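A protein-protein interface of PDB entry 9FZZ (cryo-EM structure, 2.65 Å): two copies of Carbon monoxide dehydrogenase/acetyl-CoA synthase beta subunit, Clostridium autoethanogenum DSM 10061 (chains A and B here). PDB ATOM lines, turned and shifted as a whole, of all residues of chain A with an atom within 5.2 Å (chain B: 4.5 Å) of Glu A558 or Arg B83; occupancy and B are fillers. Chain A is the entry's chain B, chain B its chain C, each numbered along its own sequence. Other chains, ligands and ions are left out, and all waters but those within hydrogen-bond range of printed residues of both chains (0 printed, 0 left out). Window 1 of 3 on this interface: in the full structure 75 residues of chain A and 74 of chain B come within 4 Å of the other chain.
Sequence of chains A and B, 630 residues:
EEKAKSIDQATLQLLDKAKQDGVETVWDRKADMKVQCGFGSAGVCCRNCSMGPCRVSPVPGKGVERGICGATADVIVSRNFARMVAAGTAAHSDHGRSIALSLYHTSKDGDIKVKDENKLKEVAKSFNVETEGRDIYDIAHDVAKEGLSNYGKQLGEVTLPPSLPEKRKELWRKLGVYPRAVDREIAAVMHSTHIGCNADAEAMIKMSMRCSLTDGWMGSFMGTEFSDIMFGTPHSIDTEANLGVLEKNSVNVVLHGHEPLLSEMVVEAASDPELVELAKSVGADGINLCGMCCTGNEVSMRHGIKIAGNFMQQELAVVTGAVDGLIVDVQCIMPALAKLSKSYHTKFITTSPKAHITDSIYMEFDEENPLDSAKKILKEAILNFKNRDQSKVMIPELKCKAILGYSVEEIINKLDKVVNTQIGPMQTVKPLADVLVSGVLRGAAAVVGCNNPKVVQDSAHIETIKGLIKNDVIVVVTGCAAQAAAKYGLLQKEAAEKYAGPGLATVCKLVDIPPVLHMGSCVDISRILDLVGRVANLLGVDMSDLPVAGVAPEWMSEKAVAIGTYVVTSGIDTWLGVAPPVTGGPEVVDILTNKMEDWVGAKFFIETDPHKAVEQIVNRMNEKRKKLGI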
ATOM      1  N   ARG A  83      -1.004 -32.175   4.562  1.00  0.00           N
ATOM      2  CA  ARG A  83      -0.051 -31.072   4.689  1.00  0.00           C
ATOM      3  C   ARG A  83       1.064 -31.197   3.653  1.00  0.00           C
ATOM      4  O   ARG A  83       1.538 -30.183   3.126  1.00  0.00           O
ATOM      5  CB  ARG A  83       0.507 -31.003   6.119  1.00  0.00           C
ATOM      6  CG  ARG A  83      -0.529 -30.449   7.138  1.00  0.00           C
ATOM      7  CD  ARG A  83       0.113 -29.690   8.334  1.00  0.00           C
ATOM      8  NE  ARG A  83      -0.920 -29.056   9.142  1.00  0.00           N
ATOM      9  CZ  ARG A  83      -0.770 -28.500  10.334  1.00  0.00           C
ATOM     10  NH1 ARG A  83       0.388 -28.503  10.959  1.00  0.00           N
ATOM     11  NH2 ARG A  83      -1.828 -27.928  10.921  1.00  0.00           N
ATOM     12  N   MET A  84       1.490 -32.420   3.334  1.00  0.00           N
ATOM     13  CA  MET A  84       2.453 -32.568   2.235  1.00  0.00           C
ATOM     14  C   MET A  84       1.869 -32.048   0.924  1.00  0.00           C
ATOM     15  O   MET A  84       2.542 -31.324   0.171  1.00  0.00           O
ATOM     16  CB  MET A  84       2.863 -34.029   2.063  1.00  0.00           C
ATOM     17  CG  MET A  84       3.546 -34.603   3.282  1.00  0.00           C
ATOM     18  SD  MET A  84       4.219 -36.239   2.940  1.00  0.00           S
ATOM     19  CE  MET A  84       5.644 -35.839   1.945  1.00  0.00           C
ATOM     20  N   VAL A  85       0.613 -32.401   0.642  1.00  0.00           N
ATOM     21  CA  VAL A  85      -0.038 -31.916  -0.577  1.00  0.00           C
ATOM     22  C   VAL A  85      -0.120 -30.392  -0.571  1.00  0.00           C
ATOM     23  O   VAL A  85       0.139 -29.737  -1.588  1.00  0.00           O
ATOM     24  CB  VAL A  85      -1.430 -32.559  -0.739  1.00  0.00           C
ATOM     25  CG1 VAL A  85      -2.253 -31.809  -1.787  1.00  0.00           C
ATOM     26  CG2 VAL A  85      -1.319 -34.065  -1.104  1.00  0.00           C
ATOM     27  N   ALA A  87       1.809 -28.230   0.977  1.00  0.00           N
ATOM     28  CA  ALA A  87       3.130 -27.646   0.762  1.00  0.00           C
ATOM     29  C   ALA A  87       3.544 -27.712  -0.711  1.00  0.00           C
ATOM     30  O   ALA A  87       4.037 -26.725  -1.275  1.00  0.00           O
ATOM     31  CB  ALA A  87       4.156 -28.356   1.648  1.00  0.00           C
ATOM     32  N   GLY A  88       3.332 -28.866  -1.359  1.00  0.00           N
ATOM     33  CA  GLY A  88       3.648 -28.977  -2.781  1.00  0.00           C
ATOM     34  C   GLY A  88       2.837 -28.017  -3.633  1.00  0.00           C
ATOM     35  O   GLY A  88       3.372 -27.343  -4.528  1.00  0.00           O
ATOM     36  N   MET A 190      -4.719 -26.305   5.448  1.00  0.00           N
ATOM     37  CA  MET A 190      -4.013 -25.974   6.688  1.00  0.00           C
ATOM     38  C   MET A 190      -4.995 -25.782   7.842  1.00  0.00           C
ATOM     39  O   MET A 190      -4.718 -26.194   8.978  1.00  0.00           O
ATOM     40  CB  MET A 190      -3.160 -24.712   6.493  1.00  0.00           C
ATOM     41  CG  MET A 190      -1.961 -24.898   5.528  1.00  0.00           C
ATOM     42  SD  MET A 190      -0.811 -26.181   6.085  1.00  0.00           S
ATOM     43  CE  MET A 190      -0.161 -25.494   7.608  1.00  0.00           C
ATOM     44  N   MET A 556      11.012 -37.395  -4.055  1.00  0.00           N
ATOM     45  CA  MET A 556      11.367 -36.989  -2.698  1.00  0.00           C
ATOM     46  C   MET A 556      10.550 -35.809  -2.161  1.00  0.00           C
ATOM     47  O   MET A 556      10.329 -35.722  -0.952  1.00  0.00           O
ATOM     48  CB  MET A 556      12.876 -36.676  -2.619  1.00  0.00           C
ATOM     49  CG  MET A 556      13.319 -35.387  -3.350  1.00  0.00           C
ATOM     50  SD  MET A 556      13.238 -33.854  -2.394  1.00  0.00           S
ATOM     51  CE  MET A 556      13.674 -32.635  -3.636  1.00  0.00           C
ATOM     52  N   SER A 557      10.092 -34.906  -3.028  1.00  0.00           N
ATOM     53  CA  SER A 557       9.591 -33.600  -2.618  1.00  0.00           C
ATOM     54  C   SER A 557       8.091 -33.626  -2.321  1.00  0.00           C
ATOM     55  O   SER A 557       7.344 -34.480  -2.800  1.00  0.00           O
ATOM     56  CB  SER A 557       9.887 -32.525  -3.677  1.00  0.00           C
ATOM     57  OG  SER A 557       9.189 -32.766  -4.898  1.00  0.00           O
ATOM     58  N   GLU A 558       7.655 -32.638  -1.538  1.00  0.00           N
ATOM     59  CA  GLU A 558       6.225 -32.422  -1.343  1.00  0.00           C
ATOM     60  C   GLU A 558       5.547 -32.073  -2.662  1.00  0.00           C
ATOM     61  O   GLU A 558       4.394 -32.464  -2.898  1.00  0.00           O
ATOM     62  CB  GLU A 558       6.000 -31.322  -0.290  1.00  0.00           C
ATOM     63  CG  GLU A 558       6.297 -31.806   1.152  1.00  0.00           C
ATOM     64  CD  GLU A 558       6.465 -30.661   2.163  1.00  0.00           C
ATOM     65  OE1 GLU A 558       7.053 -29.621   1.813  1.00  0.00           O
ATOM     66  OE2 GLU A 558       5.996 -30.806   3.309  1.00  0.00           O
ATOM     67  N   LYS A 559       6.259 -31.382  -3.553  1.00  0.00           N
ATOM     68  CA  LYS A 559       5.718 -31.129  -4.883  1.00  0.00           C
ATOM     69  C   LYS A 559       5.364 -32.425  -5.605  1.00  0.00           C
ATOM     70  O   LYS A 559       4.299 -32.524  -6.217  1.00  0.00           O
ATOM     71  CB  LYS A 559       6.723 -30.333  -5.716  1.00  0.00           C
ATOM     72  CG  LYS A 559       6.725 -28.830  -5.430  1.00  0.00           C
ATOM     73  CD  LYS A 559       7.752 -28.091  -6.323  1.00  0.00           C
ATOM     74  CE  LYS A 559       9.207 -28.474  -5.943  1.00  0.00           C
ATOM     75  NZ  LYS A 559      10.250 -27.906  -6.876  1.00  0.00           N
ATOM     76  N   ALA A 560       6.194 -33.457  -5.466  1.00  0.00           N
ATOM     77  CA  ALA A 560       5.889 -34.747  -6.083  1.00  0.00           C
ATOM     78  C   ALA A 560       4.609 -35.345  -5.517  1.00  0.00           C
ATOM     79  O   ALA A 560       3.807 -35.927  -6.259  1.00  0.00           O
ATOM     80  CB  ALA A 560       7.066 -35.706  -5.902  1.00  0.00           C
ATOM     81  N   VAL A 561       4.386 -35.194  -4.212  1.00  0.00           N
ATOM     82  CA  VAL A 561       3.156 -35.693  -3.601  1.00  0.00           C
ATOM     83  C   VAL A 561       1.951 -34.980  -4.192  1.00  0.00           C
ATOM     84  O   VAL A 561       0.973 -35.610  -4.612  1.00  0.00           O
ATOM     85  CB  VAL A 561       3.202 -35.543  -2.072  1.00  0.00           C
ATOM     86  CG1 VAL A 561       1.870 -35.990  -1.458  1.00  0.00           C
ATOM     87  CG2 VAL A 561       4.365 -36.343  -1.494  1.00  0.00           C
ATOM     88  N   ALA A 562       2.018 -33.652  -4.272  1.00  0.00           N
ATOM     89  CA  ALA A 562       0.903 -32.899  -4.852  1.00  0.00           C
ATOM     90  C   ALA A 562       0.669 -33.293  -6.308  1.00  0.00           C
ATOM     91  O   ALA A 562      -0.486 -33.418  -6.747  1.00  0.00           O
ATOM     92  CB  ALA A 562       1.162 -31.392  -4.732  1.00  0.00           C
ATOM     93  N   ILE A 563       1.746 -33.514  -7.067  1.00  0.00           N
ATOM     94  CA  ILE A 563       1.635 -33.897  -8.475  1.00  0.00           C
ATOM     95  C   ILE A 563       0.933 -35.237  -8.617  1.00  0.00           C
ATOM     96  O   ILE A 563      -0.022 -35.378  -9.386  1.00  0.00           O
ATOM     97  CB  ILE A 563       3.026 -33.940  -9.131  1.00  0.00           C
ATOM     98  CG1 ILE A 563       3.570 -32.528  -9.358  1.00  0.00           C
ATOM     99  CG2 ILE A 563       3.000 -34.718 -10.477  1.00  0.00           C
ATOM    100  CD1 ILE A 563       5.064 -32.521  -9.612  1.00  0.00           C
ATOM    101  N   ASN B  48       9.784 -32.836   6.190  1.00  0.00           N
ATOM    102  CA  ASN B  48       9.298 -32.040   5.072  1.00  0.00           C
ATOM    103  C   ASN B  48       9.507 -32.693   3.709  1.00  0.00           C
ATOM    104  O   ASN B  48       8.903 -32.234   2.739  1.00  0.00           O
ATOM    105  CB  ASN B  48       9.949 -30.653   5.110  1.00  0.00           C
ATOM    106  CG  ASN B  48       9.399 -29.779   6.243  1.00  0.00           C
ATOM    107  OD1 ASN B  48       8.758 -30.297   7.145  1.00  0.00           O
ATOM    108  ND2 ASN B  48       9.643 -28.468   6.197  1.00  0.00           N
ATOM    109  N   ARG B  79      11.762 -23.669  10.364  1.00  0.00           N
ATOM    110  CA  ARG B  79      10.700 -24.111   9.458  1.00  0.00           C
ATOM    111  C   ARG B  79       9.518 -24.701  10.226  1.00  0.00           C
ATOM    112  O   ARG B  79       8.359 -24.379   9.934  1.00  0.00           O
ATOM    113  CB  ARG B  79      11.254 -25.103   8.428  1.00  0.00           C
ATOM    114  CG  ARG B  79      12.271 -24.444   7.449  1.00  0.00           C
ATOM    115  CD  ARG B  79      12.647 -25.362   6.265  1.00  0.00           C
ATOM    116  NE  ARG B  79      13.162 -26.657   6.693  1.00  0.00           N
ATOM    117  CZ  ARG B  79      13.741 -27.535   5.885  1.00  0.00           C
ATOM    118  NH1 ARG B  79      13.967 -27.258   4.615  1.00  0.00           N
ATOM    119  NH2 ARG B  79      14.098 -28.731   6.366  1.00  0.00           N
ATOM    120  N   ASN B  80       9.787 -25.517  11.254  1.00  0.00           N
ATOM    121  CA  ASN B  80       8.698 -26.064  12.066  1.00  0.00           C
ATOM    122  C   ASN B  80       7.894 -24.946  12.727  1.00  0.00           C
ATOM    123  O   ASN B  80       6.651 -24.954  12.707  1.00  0.00           O
ATOM    124  CB  ASN B  80       9.262 -27.015  13.127  1.00  0.00           C
ATOM    125  CG  ASN B  80       9.803 -28.330  12.541  1.00  0.00           C
ATOM    126  OD1 ASN B  80       9.401 -28.731  11.461  1.00  0.00           O
ATOM    127  ND2 ASN B  80      10.705 -28.996  13.259  1.00  0.00           N
ATOM    128  N   PHE B  81       8.587 -23.958  13.284  1.00  0.00           N
ATOM    129  CA  PHE B  81       7.899 -22.828  13.902  1.00  0.00           C
ATOM    130  C   PHE B  81       7.051 -22.064  12.887  1.00  0.00           C
ATOM    131  O   PHE B  81       5.881 -21.740  13.148  1.00  0.00           O
ATOM    132  CB  PHE B  81       8.919 -21.897  14.562  1.00  0.00           C
ATOM    133  CG  PHE B  81       8.298 -20.723  15.274  1.00  0.00           C
ATOM    134  CD1 PHE B  81       7.913 -20.837  16.612  1.00  0.00           C
ATOM    135  CD2 PHE B  81       8.085 -19.509  14.609  1.00  0.00           C
ATOM    136  CE1 PHE B  81       7.317 -19.756  17.294  1.00  0.00           C
ATOM    137  CE2 PHE B  81       7.488 -18.412  15.279  1.00  0.00           C
ATOM    138  CZ  PHE B  81       7.107 -18.543  16.626  1.00  0.00           C
ATOM    139  N   ALA B  82       7.605 -21.823  11.698  1.00  0.00           N
ATOM    140  CA  ALA B  82       6.884 -21.101  10.654  1.00  0.00           C
ATOM    141  C   ALA B  82       5.626 -21.842  10.230  1.00  0.00           C
ATOM    142  O   ALA B  82       4.577 -21.224  10.013  1.00  0.00           O
ATOM    143  CB  ALA B  82       7.798 -20.857   9.453  1.00  0.00           C
ATOM    144  N   ARG B  83       5.695 -23.167  10.140  1.00  0.00           N
ATOM    145  CA  ARG B  83       4.515 -23.943   9.756  1.00  0.00           C
ATOM    146  C   ARG B  83       3.455 -23.895  10.854  1.00  0.00           C
ATOM    147  O   ARG B  83       2.254 -23.852  10.558  1.00  0.00           O
ATOM    148  CB  ARG B  83       4.914 -25.386   9.404  1.00  0.00           C
ATOM    149  CG  ARG B  83       5.650 -25.488   8.034  1.00  0.00           C
ATOM    150  CD  ARG B  83       5.441 -26.849   7.306  1.00  0.00           C
ATOM    151  NE  ARG B  83       6.002 -26.798   5.962  1.00  0.00           N
ATOM    152  CZ  ARG B  83       6.141 -27.811   5.120  1.00  0.00           C
ATOM    153  NH1 ARG B  83       5.800 -29.039   5.448  1.00  0.00           N
ATOM    154  NH2 ARG B  83       6.649 -27.578   3.904  1.00  0.00           N
ATOM    155  N   MET B  84       3.866 -23.875  12.122  1.00  0.00           N
ATOM    156  CA  MET B  84       2.870 -23.681  13.181  1.00  0.00           C
ATOM    157  C   MET B  84       2.167 -22.335  13.021  1.00  0.00           C
ATOM    158  O   MET B  84       0.932 -22.245  13.137  1.00  0.00           O
ATOM    159  CB  MET B  84       3.521 -23.755  14.560  1.00  0.00           C
ATOM    160  CG  MET B  84       4.153 -25.097  14.844  1.00  0.00           C
ATOM    161  SD  MET B  84       4.699 -25.211  16.557  1.00  0.00           S
ATOM    162  CE  MET B  84       3.152 -25.431  17.416  1.00  0.00           C
ATOM    163  N   VAL B  85       2.937 -21.280  12.746  1.00  0.00           N
ATOM    164  CA  VAL B  85       2.336 -19.961  12.541  1.00  0.00           C
ATOM    165  C   VAL B  85       1.379 -19.983  11.350  1.00  0.00           C
ATOM    166  O   VAL B  85       0.282 -19.419  11.406  1.00  0.00           O
ATOM    167  CB  VAL B  85       3.432 -18.892  12.367  1.00  0.00           C
ATOM    168  CG1 VAL B  85       2.839 -17.591  11.825  1.00  0.00           C
ATOM    169  CG2 VAL B  85       4.189 -18.637  13.700  1.00  0.00           C
ATOM    170  N   ALA B  86       1.781 -20.632  10.252  1.00  0.00           N
ATOM    171  CA  ALA B  86       0.933 -20.687   9.063  1.00  0.00           C
ATOM    172  C   ALA B  86      -0.365 -21.424   9.346  1.00  0.00           C
ATOM    173  O   ALA B  86      -1.436 -21.005   8.898  1.00  0.00           O
ATOM    174  CB  ALA B  86       1.684 -21.347   7.901  1.00  0.00           C
ATOM    175  N   ALA B  87      -0.299 -22.518  10.100  1.00  0.00           N
ATOM    176  CA  ALA B  87      -1.515 -23.253  10.438  1.00  0.00           C
ATOM    177  C   ALA B  87      -2.457 -22.415  11.308  1.00  0.00           C
ATOM    178  O   ALA B  87      -3.670 -22.361  11.056  1.00  0.00           O
ATOM    179  CB  ALA B  87      -1.146 -24.564  11.137  1.00  0.00           C
ATOM    180  N   VAL B 189       4.587 -18.802   3.267  1.00  0.00           N
ATOM    181  CA  VAL B 189       5.244 -19.546   4.339  1.00  0.00           C
ATOM    182  C   VAL B 189       5.346 -21.023   3.972  1.00  0.00           C
ATOM    183  O   VAL B 189       6.408 -21.641   4.107  1.00  0.00           O
ATOM    184  CB  VAL B 189       4.509 -19.350   5.675  1.00  0.00           C
ATOM    185  CG1 VAL B 189       5.010 -20.387   6.705  1.00  0.00           C
ATOM    186  CG2 VAL B 189       4.674 -17.901   6.189  1.00  0.00           C
ATOM    187  N   MET B 190       4.260 -21.603   3.454  1.00  0.00           N
ATOM    188  CA  MET B 190       4.322 -23.015   3.060  1.00  0.00           C
ATOM    189  C   MET B 190       5.334 -23.237   1.938  1.00  0.00           C
ATOM    190  O   MET B 190       6.012 -24.274   1.913  1.00  0.00           O
ATOM    191  CB  MET B 190       2.933 -23.513   2.627  1.00  0.00           C
ATOM    192  CG  MET B 190       1.889 -23.572   3.771  1.00  0.00           C
ATOM    193  SD  MET B 190       2.400 -24.655   5.131  1.00  0.00           S
ATOM    194  CE  MET B 190       2.423 -26.275   4.363  1.00  0.00           C
ATOM    195  N   THR B 193       9.155 -23.145   3.363  1.00  0.00           N
ATOM    196  CA  THR B 193       9.555 -24.295   4.170  1.00  0.00           C
ATOM    197  C   THR B 193       9.741 -25.575   3.349  1.00  0.00           C
ATOM    198  O   THR B 193      10.237 -26.568   3.888  1.00  0.00           O
ATOM    199  CB  THR B 193       8.541 -24.550   5.294  1.00  0.00           C
ATOM    200  OG1 THR B 193       7.237 -24.723   4.731  1.00  0.00           O
ATOM    201  CG2 THR B 193       8.526 -23.377   6.297  1.00  0.00           C
ATOM    202  N   HIS B 194       9.370 -25.573   2.067  1.00  0.00           N
ATOM    203  CA  HIS B 194       9.590 -26.732   1.206  1.00  0.00           C
ATOM    204  C   HIS B 194      11.080 -27.072   1.114  1.00  0.00           C
ATOM    205  O   HIS B 194      11.941 -26.194   1.206  1.00  0.00           O
ATOM    206  CB  HIS B 194       9.021 -26.429  -0.187  1.00  0.00           C
ATOM    207  CG  HIS B 194       9.080 -27.584  -1.143  1.00  0.00           C
ATOM    208  ND1 HIS B 194      10.223 -27.958  -1.790  1.00  0.00           N
ATOM    209  CD2 HIS B 194       8.114 -28.435  -1.569  1.00  0.00           C
ATOM    210  CE1 HIS B 194       9.982 -28.999  -2.568  1.00  0.00           C
ATOM    211  NE2 HIS B 194       8.699 -29.304  -2.449  1.00  0.00           N
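Of the printed residues of chain B, Arg A83 touches Ala B87 (3.4 Å). Printed residues of chain B within 4 Å of Met A190: Ala B87 and Met B190. Of the printed residues of chain B, Glu A558 touches Asn B48 (3.0 Å), Arg B83 (2.8 Å) and His B194 (3.6 Å). Of the printed residues of chain B, Lys A559 touches His B194 (3.4 Å). Of chain A, only Ala A87 (3.5 Å) and Glu A558 (2.8 Å) come within 4 Å of Arg B83. Of the printed residues of chain A, Ala B87 touches Arg A83 (3.4 Å) and Met A190 (3.8 Å). Of the printed residues of chain A, Met B190 touches Ala A87 (3.8 Å) and Met A190 (3.7 Å). The nearest printed residue of chain B that does not touch Met A190 is Arg B83 (4.2 Å).
NH2 of Arg A83 touches CB of Ala B87 (3.4 Å). Arg B83 touches Ala A87 (NH2 to CB, 3.5 Å). Met B190 touches Ala A87. Ala B87 touches Met A190. Ser A557 touches His B194. Glu A558 touches His B194 (N to NE2, 3.6 Å).
The side-chain carboxylate (OE2) of Glu A558 sits close to the backbone carbonyl oxygen (O) of Asn B48 (3.3 Å). The side-chain sulfur (SD) of Met B190 sits close to the side-chain sulfur (SD) of Met A190 (3.7 Å). N of Lys A559 is in hydrogen-bond range of NE2 of His B194 (3.4 Å). NH1 of Arg B83 lies within salt-bridge range of OE2 of Glu A558 (2.8 Å).
Of the 14 printed residues of chain A, 6 touch a printed residue of chain B. Printed residues of chain A that touch a printed residue of chain B: Arg A83, Ala A87, Met A190, Ser A557, Glu A558 and Lys A559. Hydrophobic or aromatic side chains of chain A that line the printed part of chain B: Ala A87 and Met A190. Printed residues of chain B that touch a printed residue of chain A: Asn B48, Arg B83, Ala B87, Met B190 and His B194. Hydrophobic or aromatic side chains of chain B within 4 Å of the printed part of chain A: Ala B87, Met B190 and His B194. Among the printed residues, 10 pairs touch across the chains.
The side-chain amide nitrogen of Asn B48 lies within hydrogen-bond range of the backbone carbonyl oxygen of Thr B193. NE of Arg B83 sits at hydrogen-bond distance from OG1 of Thr B193. The side-chain hydroxyl (OG) of Ser A557 is in hydrogen-bond range of the backbone NH (N) of Ala A560, at 3.1 Å. O of Met B190 is in hydrogen-bond range of OG1 of Thr B193, 3.1 Å away.
Arg A83 touches Ala B87, and with the chains exchanged Ala A87 touches Arg B83. Ala A87 touches Met B190, and with the chains exchanged Met A190 touches Ala B87. Met A190 touches its own counterpart, Met B190. Positions printed for both chains: 83, 84, 85, 87 and 190. Of the 10 pairs that touch across the chains among the printed residues, 5 have their exchanged pair printed and touching as well.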
